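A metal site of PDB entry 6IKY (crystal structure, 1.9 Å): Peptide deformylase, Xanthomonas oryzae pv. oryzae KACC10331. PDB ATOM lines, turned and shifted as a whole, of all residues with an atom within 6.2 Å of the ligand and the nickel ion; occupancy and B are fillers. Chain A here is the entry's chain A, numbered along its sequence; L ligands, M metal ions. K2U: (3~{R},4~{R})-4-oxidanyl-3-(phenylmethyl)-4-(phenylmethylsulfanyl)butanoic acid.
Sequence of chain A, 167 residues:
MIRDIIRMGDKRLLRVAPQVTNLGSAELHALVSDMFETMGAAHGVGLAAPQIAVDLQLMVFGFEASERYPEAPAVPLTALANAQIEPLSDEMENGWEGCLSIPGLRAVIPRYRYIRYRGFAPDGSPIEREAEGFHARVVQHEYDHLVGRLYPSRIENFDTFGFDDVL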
ATOM      1  N   MET A  39      38.056 -16.435  11.545  1.00  0.00           N
ATOM      2  CA  MET A  39      36.738 -16.397  10.900  1.00  0.00           C
ATOM      3  C   MET A  39      35.986 -17.755  11.061  1.00  0.00           C
ATOM      4  O   MET A  39      34.803 -17.767  11.369  1.00  0.00           O
ATOM      5  CB  MET A  39      36.882 -16.018   9.426  1.00  0.00           C
ATOM      6  CG  MET A  39      35.574 -15.900   8.677  1.00  0.00           C
ATOM      7  SD  MET A  39      35.680 -15.313   6.982  1.00  0.00           S
ATOM      8  CE  MET A  39      35.863 -16.751   5.980  1.00  0.00           C
ATOM      9  N   ALA A  42      34.767 -18.443  14.695  1.00  0.00           N
ATOM     10  CA  ALA A  42      33.642 -17.595  14.987  1.00  0.00           C
ATOM     11  C   ALA A  42      32.436 -17.935  14.085  1.00  0.00           C
ATOM     12  O   ALA A  42      31.436 -17.282  14.238  1.00  0.00           O
ATOM     13  CB  ALA A  42      34.043 -16.138  14.778  1.00  0.00           C
ATOM     14  N   HIS A  43      32.553 -18.848  13.138  1.00  0.00           N
ATOM     15  CA  HIS A  43      31.475 -19.168  12.193  1.00  0.00           C
ATOM     16  C   HIS A  43      31.055 -17.932  11.370  1.00  0.00           C
ATOM     17  O   HIS A  43      29.897 -17.730  11.028  1.00  0.00           O
ATOM     18  CB  HIS A  43      30.270 -19.826  12.888  1.00  0.00           C
ATOM     19  CG  HIS A  43      30.572 -21.120  13.615  1.00  0.00           C
ATOM     20  ND1 HIS A  43      29.568 -21.969  14.008  1.00  0.00           N
ATOM     21  CD2 HIS A  43      31.727 -21.697  14.045  1.00  0.00           C
ATOM     22  CE1 HIS A  43      30.081 -23.002  14.650  1.00  0.00           C
ATOM     23  NE2 HIS A  43      31.393 -22.900  14.645  1.00  0.00           N
ATOM     24  N   GLY A  44      32.025 -17.125  10.970  1.00  0.00           N
ATOM     25  CA  GLY A  44      31.756 -16.003  10.053  1.00  0.00           C
ATOM     26  C   GLY A  44      31.807 -16.339   8.581  1.00  0.00           C
ATOM     27  O   GLY A  44      32.317 -17.381   8.238  1.00  0.00           O
ATOM     28  N   VAL A  45      31.239 -15.474   7.722  1.00  0.00           N
ATOM     29  CA  VAL A  45      31.470 -15.501   6.275  1.00  0.00           C
ATOM     30  C   VAL A  45      32.429 -14.373   5.773  1.00  0.00           C
ATOM     31  O   VAL A  45      32.737 -14.250   4.577  1.00  0.00           O
ATOM     32  CB  VAL A  45      30.141 -15.477   5.478  1.00  0.00           C
ATOM     33  CG1 VAL A  45      29.298 -16.713   5.838  1.00  0.00           C
ATOM     34  CG2 VAL A  45      29.423 -14.184   5.726  1.00  0.00           C
ATOM     35  N   GLY A  46      32.846 -13.508   6.673  1.00  0.00           N
ATOM     36  CA  GLY A  46      33.747 -12.437   6.326  1.00  0.00           C
ATOM     37  C   GLY A  46      34.424 -12.026   7.610  1.00  0.00           C
ATOM     38  O   GLY A  46      33.878 -12.257   8.697  1.00  0.00           O
ATOM     39  N   LEU A  47      35.583 -11.424   7.512  1.00  0.00           N
ATOM     40  CA  LEU A  47      36.265 -10.842   8.661  1.00  0.00           C
ATOM     41  C   LEU A  47      37.239  -9.763   8.157  1.00  0.00           C
ATOM     42  O   LEU A  47      38.041 -10.020   7.227  1.00  0.00           O
ATOM     43  CB  LEU A  47      37.011 -11.948   9.399  1.00  0.00           C
ATOM     44  CG  LEU A  47      37.798 -11.425  10.615  1.00  0.00           C
ATOM     45  CD1 LEU A  47      36.902 -11.048  11.796  1.00  0.00           C
ATOM     46  CD2 LEU A  47      38.873 -12.403  11.078  1.00  0.00           C
ATOM     47  N   ALA A  48      37.237  -8.585   8.757  1.00  0.00           N
ATOM     48  CA  ALA A  48      38.151  -7.533   8.312  1.00  0.00           C
ATOM     49  C   ALA A  48      39.217  -7.388   9.339  1.00  0.00           C
ATOM     50  O   ALA A  48      39.012  -7.604  10.506  1.00  0.00           O
ATOM     51  CB  ALA A  48      37.424  -6.213   8.052  1.00  0.00           C
ATOM     52  N   GLN A  51      38.703  -5.808  12.785  1.00  0.00           N
ATOM     53  CA  GLN A  51      38.016  -6.565  13.815  1.00  0.00           C
ATOM     54  C   GLN A  51      38.913  -7.389  14.744  1.00  0.00           C
ATOM     55  O   GLN A  51      38.451  -7.799  15.814  1.00  0.00           O
ATOM     56  CB  GLN A  51      36.964  -7.523  13.229  1.00  0.00           C
ATOM     57  CG  GLN A  51      35.882  -6.803  12.463  1.00  0.00           C
ATOM     58  CD  GLN A  51      34.876  -7.752  11.820  1.00  0.00           C
ATOM     59  OE1 GLN A  51      35.095  -8.211  10.693  1.00  0.00           O
ATOM     60  NE2 GLN A  51      33.773  -8.061  12.538  1.00  0.00           N
ATOM     61  N   TRP A  96      19.341  -9.507   5.306  1.00  0.00           N
ATOM     62  CA  TRP A  96      19.814  -9.651   6.695  1.00  0.00           C
ATOM     63  C   TRP A  96      21.367  -9.565   6.860  1.00  0.00           C
ATOM     64  O   TRP A  96      22.145 -10.171   6.093  1.00  0.00           O
ATOM     65  CB  TRP A  96      19.306 -10.971   7.266  1.00  0.00           C
ATOM     66  CG  TRP A  96      17.810 -11.016   7.508  1.00  0.00           C
ATOM     67  CD1 TRP A  96      16.842 -11.686   6.789  1.00  0.00           C
ATOM     68  CD2 TRP A  96      17.120 -10.337   8.590  1.00  0.00           C
ATOM     69  NE1 TRP A  96      15.583 -11.440   7.367  1.00  0.00           N
ATOM     70  CE2 TRP A  96      15.737 -10.637   8.465  1.00  0.00           C
ATOM     71  CE3 TRP A  96      17.541  -9.483   9.627  1.00  0.00           C
ATOM     72  CZ2 TRP A  96      14.764 -10.104   9.370  1.00  0.00           C
ATOM     73  CZ3 TRP A  96      16.597  -8.996  10.512  1.00  0.00           C
ATOM     74  CH2 TRP A  96      15.203  -9.306  10.361  1.00  0.00           C
ATOM     75  N   GLU A  97      21.826  -8.877   7.900  1.00  0.00           N
ATOM     76  CA  GLU A  97      23.242  -8.913   8.251  1.00  0.00           C
ATOM     77  C   GLU A  97      23.409  -9.046   9.732  1.00  0.00           C
ATOM     78  O   GLU A  97      22.563  -8.546  10.523  1.00  0.00           O
ATOM     79  CB  GLU A  97      23.996  -7.639   7.807  1.00  0.00           C
ATOM     80  CG  GLU A  97      23.880  -7.409   6.298  1.00  0.00           C
ATOM     81  CD  GLU A  97      24.728  -6.262   5.697  1.00  0.00           C
ATOM     82  OE1 GLU A  97      25.609  -5.691   6.373  1.00  0.00           O
ATOM     83  OE2 GLU A  97      24.466  -5.883   4.496  1.00  0.00           O
ATOM     84  N   GLY A  98      24.509  -9.669  10.106  1.00  0.00           N
ATOM     85  CA  GLY A  98      25.018  -9.614  11.451  1.00  0.00           C
ATOM     86  C   GLY A  98      26.518  -9.310  11.344  1.00  0.00           C
ATOM     87  O   GLY A  98      27.044  -9.122  10.245  1.00  0.00           O
ATOM     88  N   CSD A  99      27.182  -9.267  12.474  1.00  0.00           N
ATOM     89  CA  CSD A  99      28.573  -8.875  12.563  1.00  0.00           C
ATOM     90  CB  CSD A  99      28.624  -7.344  12.667  1.00  0.00           C
ATOM     91  SG  CSD A  99      30.154  -6.591  12.356  1.00  0.00           S
ATOM     92  C   CSD A  99      29.139  -9.547  13.797  1.00  0.00           C
ATOM     93  O   CSD A  99      28.530  -9.531  14.859  1.00  0.00           O
ATOM     94  OD1 CSD A  99      30.992  -7.274  13.324  1.00  0.00           O
ATOM     95  OD2 CSD A  99      30.259  -5.397  13.444  1.00  0.00           O
ATOM     96  N   LEU A 100      30.339 -10.124  13.660  1.00  0.00           N
ATOM     97  CA  LEU A 100      31.035 -10.761  14.766  1.00  0.00           C
ATOM     98  C   LEU A 100      31.448  -9.791  15.874  1.00  0.00           C
ATOM     99  O   LEU A 100      31.689 -10.201  16.991  1.00  0.00           O
ATOM    100  CB  LEU A 100      32.300 -11.494  14.243  1.00  0.00           C
ATOM    101  CG  LEU A 100      31.965 -12.601  13.245  1.00  0.00           C
ATOM    102  CD1 LEU A 100      33.187 -12.997  12.399  1.00  0.00           C
ATOM    103  CD2 LEU A 100      31.282 -13.734  13.982  1.00  0.00           C
ATOM    104  N   SER A 101      31.625  -8.515  15.554  1.00  0.00           N
ATOM    105  CA  SER A 101      31.909  -7.522  16.576  1.00  0.00           C
ATOM    106  C   SER A 101      30.593  -7.024  17.271  1.00  0.00           C
ATOM    107  O   SER A 101      30.632  -6.189  18.170  1.00  0.00           O
ATOM    108  CB  SER A 101      32.643  -6.347  15.959  1.00  0.00           C
ATOM    109  OG  SER A 101      33.908  -6.760  15.379  1.00  0.00           O
ATOM    110  N   PHE A 134      24.476 -11.839  -2.450  1.00  0.00           N
ATOM    111  CA  PHE A 134      25.108 -12.146  -1.173  1.00  0.00           C
ATOM    112  C   PHE A 134      26.624 -11.948  -1.222  1.00  0.00           C
ATOM    113  O   PHE A 134      27.233 -11.229  -0.373  1.00  0.00           O
ATOM    114  CB  PHE A 134      24.714 -13.535  -0.639  1.00  0.00           C
ATOM    115  CG  PHE A 134      25.139 -13.722   0.799  1.00  0.00           C
ATOM    116  CD1 PHE A 134      24.580 -12.940   1.792  1.00  0.00           C
ATOM    117  CD2 PHE A 134      26.121 -14.606   1.168  1.00  0.00           C
ATOM    118  CE1 PHE A 134      24.975 -13.061   3.124  1.00  0.00           C
ATOM    119  CE2 PHE A 134      26.529 -14.728   2.494  1.00  0.00           C
ATOM    120  CZ  PHE A 134      25.960 -13.956   3.462  1.00  0.00           C
ATOM    121  N   ARG A 137      27.213  -8.240  -1.013  1.00  0.00           N
ATOM    122  CA  ARG A 137      26.890  -7.732   0.323  1.00  0.00           C
ATOM    123  C   ARG A 137      28.010  -7.944   1.317  1.00  0.00           C
ATOM    124  O   ARG A 137      28.353  -7.038   2.063  1.00  0.00           O
ATOM    125  CB  ARG A 137      25.672  -8.497   0.881  1.00  0.00           C
ATOM    126  CG  ARG A 137      25.295  -8.132   2.307  1.00  0.00           C
ATOM    127  CD  ARG A 137      23.953  -8.844   2.662  1.00  0.00           C
ATOM    128  NE  ARG A 137      22.864  -8.411   1.776  1.00  0.00           N
ATOM    129  CZ  ARG A 137      22.113  -7.304   1.895  1.00  0.00           C
ATOM    130  NH1 ARG A 137      22.270  -6.500   2.891  1.00  0.00           N
ATOM    131  NH2 ARG A 137      21.197  -6.980   0.963  1.00  0.00           N
ATOM    132  N   VAL A 138      28.551  -9.157   1.283  1.00  0.00           N
ATOM    133  CA  VAL A 138      29.656  -9.491   2.173  1.00  0.00           C
ATOM    134  C   VAL A 138      30.804  -8.557   1.953  1.00  0.00           C
ATOM    135  O   VAL A 138      31.389  -7.996   2.893  1.00  0.00           O
ATOM    136  CB  VAL A 138      30.122 -10.936   2.000  1.00  0.00           C
ATOM    137  CG1 VAL A 138      31.321 -11.211   2.946  1.00  0.00           C
ATOM    138  CG2 VAL A 138      29.019 -11.849   2.451  1.00  0.00           C
ATOM    139  N   HIS A 141      30.065  -5.114   3.255  1.00  0.00           N
ATOM    140  CA  HIS A 141      30.061  -5.096   4.732  1.00  0.00           C
ATOM    141  C   HIS A 141      31.509  -5.050   5.246  1.00  0.00           C
ATOM    142  O   HIS A 141      31.831  -4.233   6.071  1.00  0.00           O
ATOM    143  CB  HIS A 141      29.374  -6.365   5.224  1.00  0.00           C
ATOM    144  CG  HIS A 141      29.403  -6.525   6.708  1.00  0.00           C
ATOM    145  ND1 HIS A 141      28.290  -6.339   7.505  1.00  0.00           N
ATOM    146  CD2 HIS A 141      30.431  -6.837   7.541  1.00  0.00           C
ATOM    147  CE1 HIS A 141      28.653  -6.501   8.779  1.00  0.00           C
ATOM    148  NE2 HIS A 141      29.938  -6.823   8.824  1.00  0.00           N
ATOM    149  N   GLU A 142      32.388  -5.858   4.666  1.00  0.00           N
ATOM    150  CA  GLU A 142      33.774  -5.846   5.127  1.00  0.00           C
ATOM    151  C   GLU A 142      34.501  -4.584   4.764  1.00  0.00           C
ATOM    152  O   GLU A 142      35.328  -4.101   5.551  1.00  0.00           O
ATOM    153  CB  GLU A 142      34.520  -7.071   4.598  1.00  0.00           C
ATOM    154  CG  GLU A 142      34.033  -8.457   5.039  1.00  0.00           C
ATOM    155  CD  GLU A 142      33.658  -8.522   6.511  1.00  0.00           C
ATOM    156  OE1 GLU A 142      34.376  -7.969   7.402  1.00  0.00           O
ATOM    157  OE2 GLU A 142      32.622  -9.129   6.809  1.00  0.00           O
ATOM    158  N   HIS A 145      34.161  -1.904   7.233  1.00  0.00           N
ATOM    159  CA  HIS A 145      35.103  -1.949   8.402  1.00  0.00           C
ATOM    160  C   HIS A 145      36.422  -1.198   8.192  1.00  0.00           C
ATOM    161  O   HIS A 145      37.008  -0.574   9.096  1.00  0.00           O
ATOM    162  CB  HIS A 145      35.451  -3.375   8.731  1.00  0.00           C
ATOM    163  CG  HIS A 145      34.403  -4.102   9.490  1.00  0.00           C
ATOM    164  ND1 HIS A 145      33.982  -3.665  10.722  1.00  0.00           N
ATOM    165  CD2 HIS A 145      33.676  -5.212   9.200  1.00  0.00           C
ATOM    166  CE1 HIS A 145      33.077  -4.519  11.186  1.00  0.00           C
ATOM    167  NE2 HIS A 145      32.876  -5.445  10.287  1.00  0.00           N
ATOM    168  N   LEU A 150      30.043   0.640  10.863  1.00  0.00           N
ATOM    169  CA  LEU A 150      29.341  -0.573  11.211  1.00  0.00           C
ATOM    170  C   LEU A 150      27.901  -0.514  10.730  1.00  0.00           C
ATOM    171  O   LEU A 150      27.360   0.597  10.477  1.00  0.00           O
ATOM    172  CB  LEU A 150      29.372  -0.704  12.717  1.00  0.00           C
ATOM    173  CG  LEU A 150      30.794  -0.628  13.316  1.00  0.00           C
ATOM    174  CD1 LEU A 150      30.712  -0.419  14.805  1.00  0.00           C
ATOM    175  CD2 LEU A 150      31.504  -1.932  12.902  1.00  0.00           C
ATOM    176  N   TYR A 151      27.276  -1.670  10.627  1.00  0.00           N
ATOM    177  CA  TYR A 151      25.995  -1.738   9.962  1.00  0.00           C
ATOM    178  C   TYR A 151      24.839  -0.960  10.687  1.00  0.00           C
ATOM    179  O   TYR A 151      23.889  -0.604  10.000  1.00  0.00           O
ATOM    180  CB  TYR A 151      25.570  -3.174   9.644  1.00  0.00           C
ATOM    181  CG  TYR A 151      25.060  -3.997  10.787  1.00  0.00           C
ATOM    182  CD1 TYR A 151      23.712  -3.802  11.318  1.00  0.00           C
ATOM    183  CD2 TYR A 151      25.812  -4.998  11.338  1.00  0.00           C
ATOM    184  CE1 TYR A 151      23.269  -4.546  12.401  1.00  0.00           C
ATOM    185  CE2 TYR A 151      25.342  -5.799  12.374  1.00  0.00           C
ATOM    186  CZ  TYR A 151      24.067  -5.572  12.916  1.00  0.00           C
ATOM    187  OH  TYR A 151      23.626  -6.326  13.967  1.00  0.00           O
HETATM  188  O22 K2U L   1      32.472  -7.952   9.485  1.00  0.00           O
HETATM  189  C1  K2U L   1      31.909  -9.015   9.889  1.00  0.00           C
HETATM  190  O21 K2U L   1      31.402  -9.083  11.122  1.00  0.00           O
HETATM  191  C2  K2U L   1      31.640 -10.382   9.324  1.00  0.00           C
HETATM  192  C3  K2U L   1      30.131 -10.817   9.193  1.00  0.00           C
HETATM  193  C4  K2U L   1      29.873 -10.702   7.659  1.00  0.00           C
HETATM  194  C5  K2U L   1      28.466 -10.646   7.057  1.00  0.00           C
HETATM  195  C6  K2U L   1      28.239  -9.687   6.078  1.00  0.00           C
HETATM  196  C7  K2U L   1      27.017  -9.560   5.423  1.00  0.00           C
HETATM  197  C8  K2U L   1      25.966 -10.416   5.742  1.00  0.00           C
HETATM  198  C9  K2U L   1      26.160 -11.363   6.733  1.00  0.00           C
HETATM  199  C10 K2U L   1      27.403 -11.485   7.385  1.00  0.00           C
HETATM  200  C11 K2U L   1      29.853 -12.187   9.909  1.00  0.00           C
HETATM  201  O12 K2U L   1      30.202 -13.264   9.059  1.00  0.00           O
HETATM  202  S13 K2U L   1      28.194 -12.552  10.566  1.00  0.00           S
HETATM  203  C14 K2U L   1      27.653 -14.265  10.665  1.00  0.00           C
HETATM  204  C15 K2U L   1      26.703 -14.748   9.553  1.00  0.00           C
HETATM  205  C16 K2U L   1      25.619 -13.968   9.071  1.00  0.00           C
HETATM  206  C17 K2U L   1      24.793 -14.460   8.033  1.00  0.00           C
HETATM  207  C18 K2U L   1      25.017 -15.722   7.452  1.00  0.00           C
HETATM  208  C19 K2U L   1      26.081 -16.503   7.923  1.00  0.00           C
HETATM  209  C20 K2U L   1      26.912 -16.016   8.953  1.00  0.00           C
HETATM  210 NI    NI M   1      31.270  -7.096  10.538  1.00  0.00          NI
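OE1 of Gln 51 lies close to O22 of the ligand (2.9 Å).
An oxygen (O21) of the ligand lies close to the backbone NH (N) of Leu 100 (2.9 Å).
The backbone NH (N) of Val 45 sits at hydrogen-bond distance from an oxygen (O12) of the ligand, at 2.8 Å.
The side-chain amide oxygen of Gln 51 sits close to the side-chain carboxylate of Glu 142, at 3.4 Å.
N of Ala 48 sits at hydrogen-bond distance from OE1 of Gln 51, 2.9 Å away.
ND1 of His 141 is in hydrogen-bond range of OE1 of Glu 97 (3.0 Å).
OD1 of CSD 99 is in hydrogen-bond range of N of Ser 101.
OE2 of Glu 97 is in salt-bridge range of NH1 of Arg 137, at 2.8 Å.
NE2 of Gln 51 is in hydrogen-bond range of OD1 of CSD 99 (3.0 Å).
The side-chain carboxylate of Glu 142 sits at hydrogen-bond distance from the backbone NH of Ala 48.
The side-chain sulfur (SD) of Met 39 sits at hydrogen-bond distance from the backbone NH (N) of Gly 46, at 3.4 Å.
O of Gly 98 sits close to S13 of the ligand, at 3.6 Å.
An oxygen (O22) of the ligand sits close to the side-chain carboxylate of Glu 142 (2.8 Å).
Residues that only touch the ligand: Gly 44 (3.3 Å), Gly 46 (3.0 Å), Trp 96 (3.8 Å), Glu 97 (3.7 Å), Phe 134 (3.9 Å) and Arg 137 (3.8 Å).
Hydrophobic or aromatic side chains within 4 Å of the ligand: Val 45, Leu 100, Phe 134, His 141 and His 145.
The nearest printed residue that does not touch the ligand is His 43 (4.02 Å).
Gln 51 touches the nickel ion.
The nearest printed residue that does not touch the nickel ion is Leu 100 (4.4 Å).
O22 of the ligand binds the nickel ion, at 1.8 Å.
O21 of the ligand is bound to the nickel ion (2.1 Å).
NE2 of His 141 binds the nickel ion, at 2.2 Å.
SG of CSD 99 binds the nickel ion (2.2 Å).
The nickel ion is bound by a ring nitrogen (NE2) of His 145 (2.3 Å).
The nickel ion has five donor atoms within binding distance.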
